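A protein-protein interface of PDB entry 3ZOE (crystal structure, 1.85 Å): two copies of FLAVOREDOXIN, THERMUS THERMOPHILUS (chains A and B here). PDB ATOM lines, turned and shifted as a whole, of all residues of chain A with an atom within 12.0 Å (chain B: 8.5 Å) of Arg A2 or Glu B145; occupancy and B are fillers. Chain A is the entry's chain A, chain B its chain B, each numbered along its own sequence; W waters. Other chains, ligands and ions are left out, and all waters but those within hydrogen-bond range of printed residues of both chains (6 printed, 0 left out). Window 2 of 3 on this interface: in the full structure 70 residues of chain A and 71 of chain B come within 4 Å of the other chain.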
ATOM      1  N   MET A   1      -9.912  -3.082  30.117  1.00  0.00           N
ATOM      2  CA  MET A   1     -10.654  -4.141  29.381  1.00  0.00           C
ATOM      3  C   MET A   1      -9.668  -4.794  28.432  1.00  0.00           C
ATOM      4  O   MET A   1      -9.021  -4.088  27.667  1.00  0.00           O
ATOM      5  CB  MET A   1     -11.811  -3.535  28.611  1.00  0.00           C
ATOM      6  CG  MET A   1     -13.021  -4.453  28.397  1.00  0.00           C
ATOM      7  SD  MET A   1     -14.276  -3.465  27.529  1.00  0.00           S
ATOM      8  CE  MET A   1     -15.622  -4.638  27.405  1.00  0.00           C
ATOM      9  N   ARG A   2      -9.482  -6.111  28.550  1.00  0.00           N
ATOM     10  CA  ARG A   2      -8.640  -6.874  27.595  1.00  0.00           C
ATOM     11  C   ARG A   2      -9.227  -6.848  26.175  1.00  0.00           C
ATOM     12  O   ARG A   2     -10.435  -6.863  25.991  1.00  0.00           O
ATOM     13  CB  ARG A   2      -8.484  -8.340  28.063  1.00  0.00           C
ATOM     14  CG  ARG A   2      -8.190  -9.338  26.946  1.00  0.00           C
ATOM     15  CD  ARG A   2      -8.711 -10.744  27.237  1.00  0.00           C
ATOM     16  NE  ARG A   2      -7.894 -11.713  26.512  1.00  0.00           N
ATOM     17  CZ  ARG A   2      -8.247 -12.953  26.180  1.00  0.00           C
ATOM     18  NH1 ARG A   2      -9.450 -13.451  26.456  1.00  0.00           N
ATOM     19  NH2 ARG A   2      -7.369 -13.695  25.536  1.00  0.00           N
ATOM     20  N   SER A   3      -8.373  -6.858  25.176  1.00  0.00           N
ATOM     21  CA  SER A   3      -8.821  -7.059  23.795  1.00  0.00           C
ATOM     22  C   SER A   3      -7.842  -7.897  23.008  1.00  0.00           C
ATOM     23  O   SER A   3      -6.619  -7.893  23.298  1.00  0.00           O
ATOM     24  CB  SER A   3      -8.917  -5.720  23.084  1.00  0.00           C
ATOM     25  OG  SER A   3      -7.607  -5.185  22.877  1.00  0.00           O
ATOM     26  N   TYR A   4      -8.342  -8.572  21.982  1.00  0.00           N
ATOM     27  CA  TYR A   4      -7.459  -9.187  21.008  1.00  0.00           C
ATOM     28  C   TYR A   4      -8.110  -9.180  19.628  1.00  0.00           C
ATOM     29  O   TYR A   4      -9.349  -9.033  19.515  1.00  0.00           O
ATOM     30  CB  TYR A   4      -7.123 -10.582  21.510  1.00  0.00           C
ATOM     31  CG  TYR A   4      -8.354 -11.479  21.755  1.00  0.00           C
ATOM     32  CD1 TYR A   4      -9.003 -11.541  22.991  1.00  0.00           C
ATOM     33  CD2 TYR A   4      -8.808 -12.272  20.747  1.00  0.00           C
ATOM     34  CE1 TYR A   4     -10.082 -12.379  23.164  1.00  0.00           C
ATOM     35  CE2 TYR A   4      -9.864 -13.105  20.905  1.00  0.00           C
ATOM     36  CZ  TYR A   4     -10.496 -13.162  22.080  1.00  0.00           C
ATOM     37  OH  TYR A   4     -11.535 -14.041  22.102  1.00  0.00           O
ATOM     38  N   ARG A   5      -7.288  -9.249  18.572  1.00  0.00           N
ATOM     39  CA  ARG A   5      -7.790  -9.428  17.236  1.00  0.00           C
ATOM     40  C   ARG A   5      -8.062 -10.885  17.004  1.00  0.00           C
ATOM     41  O   ARG A   5      -7.302 -11.731  17.469  1.00  0.00           O
ATOM     42  CB  ARG A   5      -6.786  -8.967  16.160  1.00  0.00           C
ATOM     43  CG  ARG A   5      -6.710  -7.457  15.985  1.00  0.00           C
ATOM     44  CD  ARG A   5      -5.488  -7.045  15.189  1.00  0.00           C
ATOM     45  NE  ARG A   5      -5.091  -5.671  15.514  1.00  0.00           N
ATOM     46  CZ  ARG A   5      -5.686  -4.564  15.067  1.00  0.00           C
ATOM     47  NH1 ARG A   5      -6.732  -4.615  14.229  1.00  0.00           N
ATOM     48  NH2 ARG A   5      -5.203  -3.383  15.451  1.00  0.00           N
ATOM     49  N   ALA A   6      -9.106 -11.163  16.233  1.00  0.00           N
ATOM     50  CA  ALA A   6      -9.482 -12.529  15.898  1.00  0.00           C
ATOM     51  C   ALA A   6      -8.533 -13.100  14.876  1.00  0.00           C
ATOM     52  O   ALA A   6      -8.165 -12.425  13.913  1.00  0.00           O
ATOM     53  CB  ALA A   6     -10.888 -12.605  15.376  1.00  0.00           C
ATOM     54  N   GLN A   7      -8.132 -14.352  15.104  1.00  0.00           N
ATOM     55  CA  GLN A   7      -7.139 -15.040  14.248  1.00  0.00           C
ATOM     56  C   GLN A   7      -7.680 -16.385  13.756  1.00  0.00           C
ATOM     57  O   GLN A   7      -6.939 -17.260  13.301  1.00  0.00           O
ATOM     58  CB  GLN A   7      -5.868 -15.262  15.086  1.00  0.00           C
ATOM     59  CG  GLN A   7      -5.252 -13.997  15.683  1.00  0.00           C
ATOM     60  CD  GLN A   7      -4.608 -14.203  17.078  1.00  0.00           C
ATOM     61  OE1 GLN A   7      -3.810 -15.124  17.297  1.00  0.00           O
ATOM     62  NE2 GLN A   7      -4.927 -13.323  18.002  1.00  0.00           N
ATOM     63  N   GLY A   8      -8.994 -16.544  13.860  1.00  0.00           N
ATOM     64  CA  GLY A   8      -9.643 -17.798  13.619  1.00  0.00           C
ATOM     65  C   GLY A   8     -10.856 -17.927  14.524  1.00  0.00           C
ATOM     66  O   GLY A   8     -11.386 -16.938  15.000  1.00  0.00           O
ATOM     67  N   PRO A   9     -11.281 -19.162  14.799  1.00  0.00           N
ATOM     68  CA  PRO A   9     -12.363 -19.283  15.738  1.00  0.00           C
ATOM     69  C   PRO A   9     -11.988 -18.823  17.136  1.00  0.00           C
ATOM     70  O   PRO A   9     -10.823 -18.991  17.559  1.00  0.00           O
ATOM     71  CB  PRO A   9     -12.728 -20.771  15.685  1.00  0.00           C
ATOM     72  CG  PRO A   9     -11.588 -21.452  15.028  1.00  0.00           C
ATOM     73  CD  PRO A   9     -10.842 -20.446  14.220  1.00  0.00           C
ATOM     74  N   LEU A  10     -12.946 -18.212  17.840  1.00  0.00           N
ATOM     75  CA  LEU A  10     -12.674 -17.645  19.161  1.00  0.00           C
ATOM     76  C   LEU A  10     -12.513 -18.754  20.206  1.00  0.00           C
ATOM     77  O   LEU A  10     -13.147 -19.807  20.086  1.00  0.00           O
ATOM     78  CB  LEU A  10     -13.769 -16.692  19.635  1.00  0.00           C
ATOM     79  CG  LEU A  10     -14.336 -15.636  18.648  1.00  0.00           C
ATOM     80  CD1 LEU A  10     -15.174 -14.652  19.468  1.00  0.00           C
ATOM     81  CD2 LEU A  10     -13.237 -14.924  17.865  1.00  0.00           C
ATOM     82  N   PRO A  11     -11.692 -18.513  21.244  1.00  0.00           N
ATOM     83  CA  PRO A  11     -11.462 -19.456  22.360  1.00  0.00           C
ATOM     84  C   PRO A  11     -12.762 -19.896  23.024  1.00  0.00           C
ATOM     85  O   PRO A  11     -12.937 -21.043  23.433  1.00  0.00           O
ATOM     86  CB  PRO A  11     -10.644 -18.623  23.369  1.00  0.00           C
ATOM     87  CG  PRO A  11     -10.046 -17.525  22.591  1.00  0.00           C
ATOM     88  CD  PRO A  11     -10.862 -17.297  21.354  1.00  0.00           C
ATOM     89  N   GLY A  12     -13.686 -18.951  23.145  1.00  0.00           N
ATOM     90  CA  GLY A  12     -15.062 -19.279  23.428  1.00  0.00           C
ATOM     91  C   GLY A  12     -15.886 -18.242  22.695  1.00  0.00           C
ATOM     92  O   GLY A  12     -15.468 -17.097  22.587  1.00  0.00           O
ATOM     93  N   PHE A  13     -17.045 -18.634  22.178  1.00  0.00           N
ATOM     94  CA  PHE A  13     -17.939 -17.713  21.503  1.00  0.00           C
ATOM     95  C   PHE A  13     -19.241 -17.604  22.315  1.00  0.00           C
ATOM     96  O   PHE A  13     -20.317 -17.920  21.818  1.00  0.00           O
ATOM     97  CB  PHE A  13     -18.161 -18.267  20.061  1.00  0.00           C
ATOM     98  CG  PHE A  13     -18.800 -17.314  19.075  1.00  0.00           C
ATOM     99  CD1 PHE A  13     -18.529 -15.942  19.080  1.00  0.00           C
ATOM    100  CD2 PHE A  13     -19.637 -17.828  18.071  1.00  0.00           C
ATOM    101  CE1 PHE A  13     -19.074 -15.109  18.123  1.00  0.00           C
ATOM    102  CE2 PHE A  13     -20.172 -16.994  17.086  1.00  0.00           C
ATOM    103  CZ  PHE A  13     -19.906 -15.636  17.129  1.00  0.00           C
ATOM    104  N   TYR A  14     -19.132 -17.179  23.574  1.00  0.00           N
ATOM    105  CA  TYR A  14     -20.270 -17.116  24.469  1.00  0.00           C
ATOM    106  C   TYR A  14     -20.599 -15.738  25.049  1.00  0.00           C
ATOM    107  O   TYR A  14     -21.426 -15.629  25.939  1.00  0.00           O
ATOM    108  CB  TYR A  14     -20.104 -18.114  25.603  1.00  0.00           C
ATOM    109  CG  TYR A  14     -19.750 -19.468  25.110  1.00  0.00           C
ATOM    110  CD1 TYR A  14     -20.679 -20.206  24.406  1.00  0.00           C
ATOM    111  CD2 TYR A  14     -18.450 -19.988  25.281  1.00  0.00           C
ATOM    112  CE1 TYR A  14     -20.365 -21.419  23.885  1.00  0.00           C
ATOM    113  CE2 TYR A  14     -18.121 -21.231  24.768  1.00  0.00           C
ATOM    114  CZ  TYR A  14     -19.081 -21.935  24.062  1.00  0.00           C
ATOM    115  OH  TYR A  14     -18.853 -23.175  23.522  1.00  0.00           O
ATOM    116  N   HIS A  15     -19.970 -14.702  24.532  1.00  0.00           N
ATOM    117  CA  HIS A  15     -20.038 -13.333  25.132  1.00  0.00           C
ATOM    118  C   HIS A  15     -21.449 -12.787  25.136  1.00  0.00           C
ATOM    119  O   HIS A  15     -21.775 -11.950  25.949  1.00  0.00           O
ATOM    120  CB  HIS A  15     -19.142 -12.392  24.367  1.00  0.00           C
ATOM    121  CG  HIS A  15     -17.742 -12.897  24.253  1.00  0.00           C
ATOM    122  ND1 HIS A  15     -17.330 -13.756  23.243  1.00  0.00           N
ATOM    123  CD2 HIS A  15     -16.675 -12.715  25.064  1.00  0.00           C
ATOM    124  CE1 HIS A  15     -16.047 -14.037  23.420  1.00  0.00           C
ATOM    125  NE2 HIS A  15     -15.619 -13.395  24.498  1.00  0.00           N
ATOM    126  N   PHE B 102     -15.724   4.248  23.744  1.00  0.00           N
ATOM    127  CA  PHE B 102     -14.383   4.299  23.255  1.00  0.00           C
ATOM    128  C   PHE B 102     -14.319   3.698  21.867  1.00  0.00           C
ATOM    129  O   PHE B 102     -15.222   2.920  21.453  1.00  0.00           O
ATOM    130  CB  PHE B 102     -13.399   3.659  24.264  1.00  0.00           C
ATOM    131  CG  PHE B 102     -13.563   2.162  24.460  1.00  0.00           C
ATOM    132  CD1 PHE B 102     -12.903   1.274  23.649  1.00  0.00           C
ATOM    133  CD2 PHE B 102     -14.345   1.653  25.514  1.00  0.00           C
ATOM    134  CE1 PHE B 102     -13.038  -0.114  23.850  1.00  0.00           C
ATOM    135  CE2 PHE B 102     -14.472   0.302  25.721  1.00  0.00           C
ATOM    136  CZ  PHE B 102     -13.806  -0.586  24.871  1.00  0.00           C
ATOM    137  N   HIS B 105     -10.132  -1.089  17.872  1.00  0.00           N
ATOM    138  CA  HIS B 105      -8.993  -1.195  16.958  1.00  0.00           C
ATOM    139  C   HIS B 105      -9.351  -0.839  15.508  1.00  0.00           C
ATOM    140  O   HIS B 105      -8.512  -0.335  14.752  1.00  0.00           O
ATOM    141  CB  HIS B 105      -8.344  -2.600  17.016  1.00  0.00           C
ATOM    142  CG  HIS B 105      -7.858  -2.997  18.376  1.00  0.00           C
ATOM    143  ND1 HIS B 105      -6.772  -2.405  18.991  1.00  0.00           N
ATOM    144  CD2 HIS B 105      -8.321  -3.926  19.249  1.00  0.00           C
ATOM    145  CE1 HIS B 105      -6.572  -2.964  20.173  1.00  0.00           C
ATOM    146  NE2 HIS B 105      -7.507  -3.888  20.359  1.00  0.00           N
ATOM    147  N   ALA B 114     -19.426  -2.325  29.263  1.00  0.00           N
ATOM    148  CA  ALA B 114     -19.806  -3.687  28.909  1.00  0.00           C
ATOM    149  C   ALA B 114     -18.869  -4.695  29.566  1.00  0.00           C
ATOM    150  O   ALA B 114     -17.684  -4.405  29.864  1.00  0.00           O
ATOM    151  CB  ALA B 114     -19.776  -3.896  27.408  1.00  0.00           C
ATOM    152  N   TYR B 115     -19.387  -5.901  29.741  1.00  0.00           N
ATOM    153  CA  TYR B 115     -18.510  -6.995  30.132  1.00  0.00           C
ATOM    154  C   TYR B 115     -17.768  -7.671  28.979  1.00  0.00           C
ATOM    155  O   TYR B 115     -16.711  -8.344  29.202  1.00  0.00           O
ATOM    156  CB  TYR B 115     -19.271  -7.998  31.014  1.00  0.00           C
ATOM    157  CG  TYR B 115     -20.596  -8.513  30.481  1.00  0.00           C
ATOM    158  CD1 TYR B 115     -20.629  -9.503  29.501  1.00  0.00           C
ATOM    159  CD2 TYR B 115     -21.796  -8.031  30.958  1.00  0.00           C
ATOM    160  CE1 TYR B 115     -21.848  -9.981  29.015  1.00  0.00           C
ATOM    161  CE2 TYR B 115     -23.018  -8.531  30.502  1.00  0.00           C
ATOM    162  CZ  TYR B 115     -23.030  -9.501  29.518  1.00  0.00           C
ATOM    163  OH  TYR B 115     -24.213 -10.021  29.032  1.00  0.00           O
ATOM    164  N   ALA B 116     -18.282  -7.487  27.753  1.00  0.00           N
ATOM    165  CA  ALA B 116     -17.651  -7.986  26.531  1.00  0.00           C
ATOM    166  C   ALA B 116     -18.193  -7.248  25.293  1.00  0.00           C
ATOM    167  O   ALA B 116     -19.257  -6.650  25.343  1.00  0.00           O
ATOM    168  CB  ALA B 116     -17.895  -9.471  26.348  1.00  0.00           C
ATOM    169  N   ALA B 117     -17.447  -7.312  24.210  1.00  0.00           N
ATOM    170  CA  ALA B 117     -17.849  -6.680  22.943  1.00  0.00           C
ATOM    171  C   ALA B 117     -17.079  -7.180  21.787  1.00  0.00           C
ATOM    172  O   ALA B 117     -15.876  -7.542  21.888  1.00  0.00           O
ATOM    173  CB  ALA B 117     -17.699  -5.185  23.026  1.00  0.00           C
ATOM    174  N   ALA B 140     -12.345  -8.212  16.147  1.00  0.00           N
ATOM    175  CA  ALA B 140     -11.725  -8.101  17.461  1.00  0.00           C
ATOM    176  C   ALA B 140     -12.712  -8.354  18.587  1.00  0.00           C
ATOM    177  O   ALA B 140     -13.947  -8.225  18.407  1.00  0.00           O
ATOM    178  CB  ALA B 140     -11.051  -6.705  17.640  1.00  0.00           C
ATOM    179  N   VAL B 141     -12.149  -8.678  19.742  1.00  0.00           N
ATOM    180  CA  VAL B 141     -12.870  -9.087  20.941  1.00  0.00           C
ATOM    181  C   VAL B 141     -12.365  -8.269  22.117  1.00  0.00           C
ATOM    182  O   VAL B 141     -11.156  -8.074  22.268  1.00  0.00           O
ATOM    183  CB  VAL B 141     -12.642 -10.598  21.292  1.00  0.00           C
ATOM    184  CG1 VAL B 141     -13.401 -10.951  22.577  1.00  0.00           C
ATOM    185  CG2 VAL B 141     -13.037 -11.487  20.128  1.00  0.00           C
ATOM    186  N   TRP B 142     -13.304  -7.731  22.886  1.00  0.00           N
ATOM    187  CA  TRP B 142     -13.064  -7.022  24.147  1.00  0.00           C
ATOM    188  C   TRP B 142     -13.692  -7.827  25.250  1.00  0.00           C
ATOM    189  O   TRP B 142     -14.838  -8.310  25.100  1.00  0.00           O
ATOM    190  CB  TRP B 142     -13.707  -5.602  24.094  1.00  0.00           C
ATOM    191  CG  TRP B 142     -12.957  -4.760  23.159  1.00  0.00           C
ATOM    192  CD1 TRP B 142     -13.061  -4.748  21.799  1.00  0.00           C
ATOM    193  CD2 TRP B 142     -11.911  -3.874  23.489  1.00  0.00           C
ATOM    194  NE1 TRP B 142     -12.169  -3.865  21.268  1.00  0.00           N
ATOM    195  CE2 TRP B 142     -11.434  -3.328  22.290  1.00  0.00           C
ATOM    196  CE3 TRP B 142     -11.314  -3.483  24.698  1.00  0.00           C
ATOM    197  CZ2 TRP B 142     -10.386  -2.402  22.250  1.00  0.00           C
ATOM    198  CZ3 TRP B 142     -10.253  -2.555  24.658  1.00  0.00           C
ATOM    199  CH2 TRP B 142      -9.806  -2.038  23.447  1.00  0.00           C
ATOM    200  N   GLU B 143     -12.987  -7.941  26.382  1.00  0.00           N
ATOM    201  CA  GLU B 143     -13.479  -8.708  27.500  1.00  0.00           C
ATOM    202  C   GLU B 143     -13.029  -8.052  28.818  1.00  0.00           C
ATOM    203  O   GLU B 143     -11.821  -7.771  29.023  1.00  0.00           O
ATOM    204  CB  GLU B 143     -12.963 -10.183  27.492  1.00  0.00           C
ATOM    205  CG  GLU B 143     -13.192 -10.991  26.207  1.00  0.00           C
ATOM    206  CD  GLU B 143     -12.765 -12.447  26.355  1.00  0.00           C
ATOM    207  OE1 GLU B 143     -11.886 -12.690  27.189  1.00  0.00           O
ATOM    208  OE2 GLU B 143     -13.317 -13.355  25.683  1.00  0.00           O
ATOM    209  N   GLU B 144     -13.998  -7.882  29.717  1.00  0.00           N
ATOM    210  CA  GLU B 144     -13.767  -7.282  31.001  1.00  0.00           C
ATOM    211  C   GLU B 144     -13.419  -8.426  31.939  1.00  0.00           C
ATOM    212  O   GLU B 144     -14.289  -9.199  32.342  1.00  0.00           O
ATOM    213  CB  GLU B 144     -14.998  -6.491  31.444  1.00  0.00           C
ATOM    214  CG  GLU B 144     -14.808  -5.668  32.705  1.00  0.00           C
ATOM    215  CD  GLU B 144     -13.634  -4.699  32.625  1.00  0.00           C
ATOM    216  OE1 GLU B 144     -13.644  -3.759  31.815  1.00  0.00           O
ATOM    217  OE2 GLU B 144     -12.698  -4.870  33.405  1.00  0.00           O
ATOM    218  N   GLU B 145     -12.130  -8.554  32.247  1.00  0.00           N
ATOM    219  CA  GLU B 145     -11.624  -9.714  32.954  1.00  0.00           C
ATOM    220  C   GLU B 145     -12.271  -9.840  34.322  1.00  0.00           C
ATOM    221  O   GLU B 145     -12.399  -8.854  35.054  1.00  0.00           O
ATOM    222  CB  GLU B 145     -10.119  -9.606  33.112  1.00  0.00           C
ATOM    223  CG  GLU B 145      -9.448  -8.956  31.925  1.00  0.00           C
ATOM    224  CD  GLU B 145      -8.361  -7.993  32.349  1.00  0.00           C
ATOM    225  OE1 GLU B 145      -8.596  -7.221  33.305  1.00  0.00           O
ATOM    226  OE2 GLU B 145      -7.275  -8.014  31.727  1.00  0.00           O
ATOM    227  N   GLY B 146     -12.715 -11.054  34.625  1.00  0.00           N
ATOM    228  CA  GLY B 146     -13.267 -11.391  35.915  1.00  0.00           C
ATOM    229  C   GLY B 146     -14.762 -11.526  35.849  1.00  0.00           C
ATOM    230  O   GLY B 146     -15.364 -11.942  36.830  1.00  0.00           O
ATOM    231  N   LEU B 147     -15.358 -11.144  34.713  1.00  0.00           N
ATOM    232  CA  LEU B 147     -16.797 -11.274  34.514  1.00  0.00           C
ATOM    233  C   LEU B 147     -17.093 -12.271  33.391  1.00  0.00           C
ATOM    234  O   LEU B 147     -18.180 -12.866  33.341  1.00  0.00           O
ATOM    235  CB  LEU B 147     -17.426  -9.906  34.227  1.00  0.00           C
ATOM    236  CG  LEU B 147     -16.857  -8.645  34.877  1.00  0.00           C
ATOM    237  CD1 LEU B 147     -17.595  -7.402  34.400  1.00  0.00           C
ATOM    238  CD2 LEU B 147     -16.890  -8.700  36.409  1.00  0.00           C
ATOM    239  N   GLY B 152     -15.172 -18.367  29.050  1.00  0.00           N
ATOM    240  CA  GLY B 152     -15.647 -17.217  28.252  1.00  0.00           C
ATOM    241  C   GLY B 152     -17.110 -16.831  28.458  1.00  0.00           C
ATOM    242  O   GLY B 152     -17.591 -15.848  27.877  1.00  0.00           O
ATOM    243  N   LYS B 155     -20.525 -13.950  33.752  1.00  0.00           N
ATOM    244  CA  LYS B 155     -20.689 -14.450  35.134  1.00  0.00           C
ATOM    245  C   LYS B 155     -22.136 -14.491  35.651  1.00  0.00           C
ATOM    246  O   LYS B 155     -23.057 -14.035  34.953  1.00  0.00           O
ATOM    247  CB  LYS B 155     -19.767 -13.683  36.089  1.00  0.00           C
ATOM    248  CG  LYS B 155     -18.410 -14.365  36.258  1.00  0.00           C
ATOM    249  CD  LYS B 155     -17.914 -14.365  37.703  1.00  0.00           C
ATOM    250  CE  LYS B 155     -17.762 -12.971  38.281  1.00  0.00           C
ATOM    251  NZ  LYS B 155     -16.550 -12.897  39.144  1.00  0.00           N
HETATM  252  O   HOH W   1     -17.090 -16.366  25.438  1.00  0.00           O
HETATM  253  O   HOH W   2     -24.077 -11.497  27.090  1.00  0.00           O
HETATM  254  O   HOH W   3     -17.427  -1.549  27.214  1.00  0.00           O
HETATM  255  O   HOH W   4      -5.627  -0.171  15.927  1.00  0.00           O
HETATM  256  O   HOH W   5     -13.810 -16.586  25.364  1.00  0.00           O
HETATM  257  O   HOH W   6     -10.056  -6.021  31.355  1.00  0.00           O
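Printed residues of chain A that touch a printed residue of chain B: Met A1, Arg A2, Ser A3, Tyr A4, Arg A5, Leu A10 and His A15.
Hydrophobic or aromatic side chains of chain A within 4 Å of the printed part of chain B: Met A1, Tyr A4, Leu A10 and His A15.
Hydrophobic or aromatic side chains of chain B within 4 Å of the printed part of chain A: Phe B102, His B105, Tyr B115, Ala B116, Ala B140, Val B141 and Trp B142.
Among the printed residues, Asp or Glu carboxylates within 4 Å of a Lys or Arg side-chain nitrogen of the other chain: Arg A2 with Glu B143.
Of the printed residues of chain B, Arg A2 touches Val B141, Trp B142, Glu B143 and Glu B145.
Of chain B, only His B105 (2.8 Å), Val B141 (3.0 Å) and Trp B142 (3.5 Å) come within 4 Å of Ser A3.
Printed residues of chain B within 4 Å of Arg A5: His B105 (3.6 Å).
Gly A12 touches none of the printed residues of chain B.
Printed residues of chain A within 4 Å of Ala B116: Met A1 (3.9 Å) and His A15 (3.7 Å).
Trp B142 touches just these residues of chain A: Met A1 (3.6 Å), Arg A2 (3.2 Å) and Ser A3 (3.5 Å).
Glu B144 touches just one residue of chain A: Met A1.
Of the printed residues of chain A, Glu B145 touches Arg A2 (3.9 Å).
No residue of chain A comes within 4 Å of Gly B146.
No residue of chain A comes within 4 Å of Leu B147.
Lys B155 touches none of the printed residues of chain A.
The nearest printed residue of chain B that does not touch Arg A2 is Glu B144 (5.0 Å).
Water W2 bridges the side-chain hydroxyl of Tyr B115 (2.4 Å) and the backbone carbonyl oxygen of His A15 (2.6 Å).
Water W1 lies within hydrogen-bond range of O of Gly B152 (2.5 Å), N of Tyr A14 (2.9 Å), O of Gly A12 (3.4 Å) and ND1 of His A15 (3.4 Å).
Water W6 lies within hydrogen-bond range of the side-chain carboxylate of Glu B145 (2.7 Å), the backbone NH of Arg A2 (2.9 Å), the backbone NH of Met A1 (3.2 Å) and the backbone carbonyl oxygen of Glu B143 (3.4 Å).
Water W3 lies within hydrogen-bond range of N of Ala B114 (3.0 Å) and SD of Met A1 (3.7 Å).
Water W4 lies within hydrogen-bond range of the backbone carbonyl oxygen of His B105 (3.1 Å) and the guanidinium group of Arg A5 (3.3 Å).
Water W5 lies within hydrogen-bond range of N of Gly A12 (3.2 Å) and OE2 of Glu B143 (3.3 Å).
NE2 of Gln A7 sits at hydrogen-bond distance from O of Arg A5 (2.9 Å).
O of Tyr B115 is in hydrogen-bond range of N of Glu B144 (2.8 Å).
The backbone NH of Trp B142 lies within hydrogen-bond range of the backbone carbonyl oxygen of Ala B117, 2.8 Å away.
Among the printed residues, merely in contact across the chains: Met A1 with Phe B102 (3.9 Å), Met A1 with Ala B114 (3.2 Å), Met A1 with Ala B116 (3.9 Å), Met A1 with Trp B142 (3.6 Å), Met A1 with Glu B143 (3.6 Å), Met A1 with Glu B144 (3.5 Å), Arg A2 with Val B141 (3.98 Å), Arg A2 with Trp B142 (3.2 Å), Arg A2 with Glu B145 (3.9 Å), Ser A3 with Val B141 (3.0 Å), Ser A3 with Trp B142 (3.5 Å), Tyr A4 with Ala B140 (3.3 Å), Arg A5 with His B105 (3.6 Å), Leu A10 with Val B141 (3.9 Å), His A15 with Tyr B115 (3.6 Å), His A15 with Ala B116 (3.7 Å) and His A15 with Val B141 (3.8 Å).
The guanidinium group (NH1) of Arg A2 lies within salt-bridge range of the side-chain carboxylate (OE1) of Glu B143, at 2.7 Å.
OG of Ser A3 lies within hydrogen-bond range of NE2 of His B105, at 2.8 Å.
O of Tyr A4 sits at hydrogen-bond distance from N of Val B141 (2.8 Å).
OE2 of Glu B143 sits at hydrogen-bond distance from NE2 of His A15 (2.6 Å).
No position is printed for both chains.
Of the 21 pairs that touch across the chains among the printed residues, none has its exchanged pair printed and touching as well.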
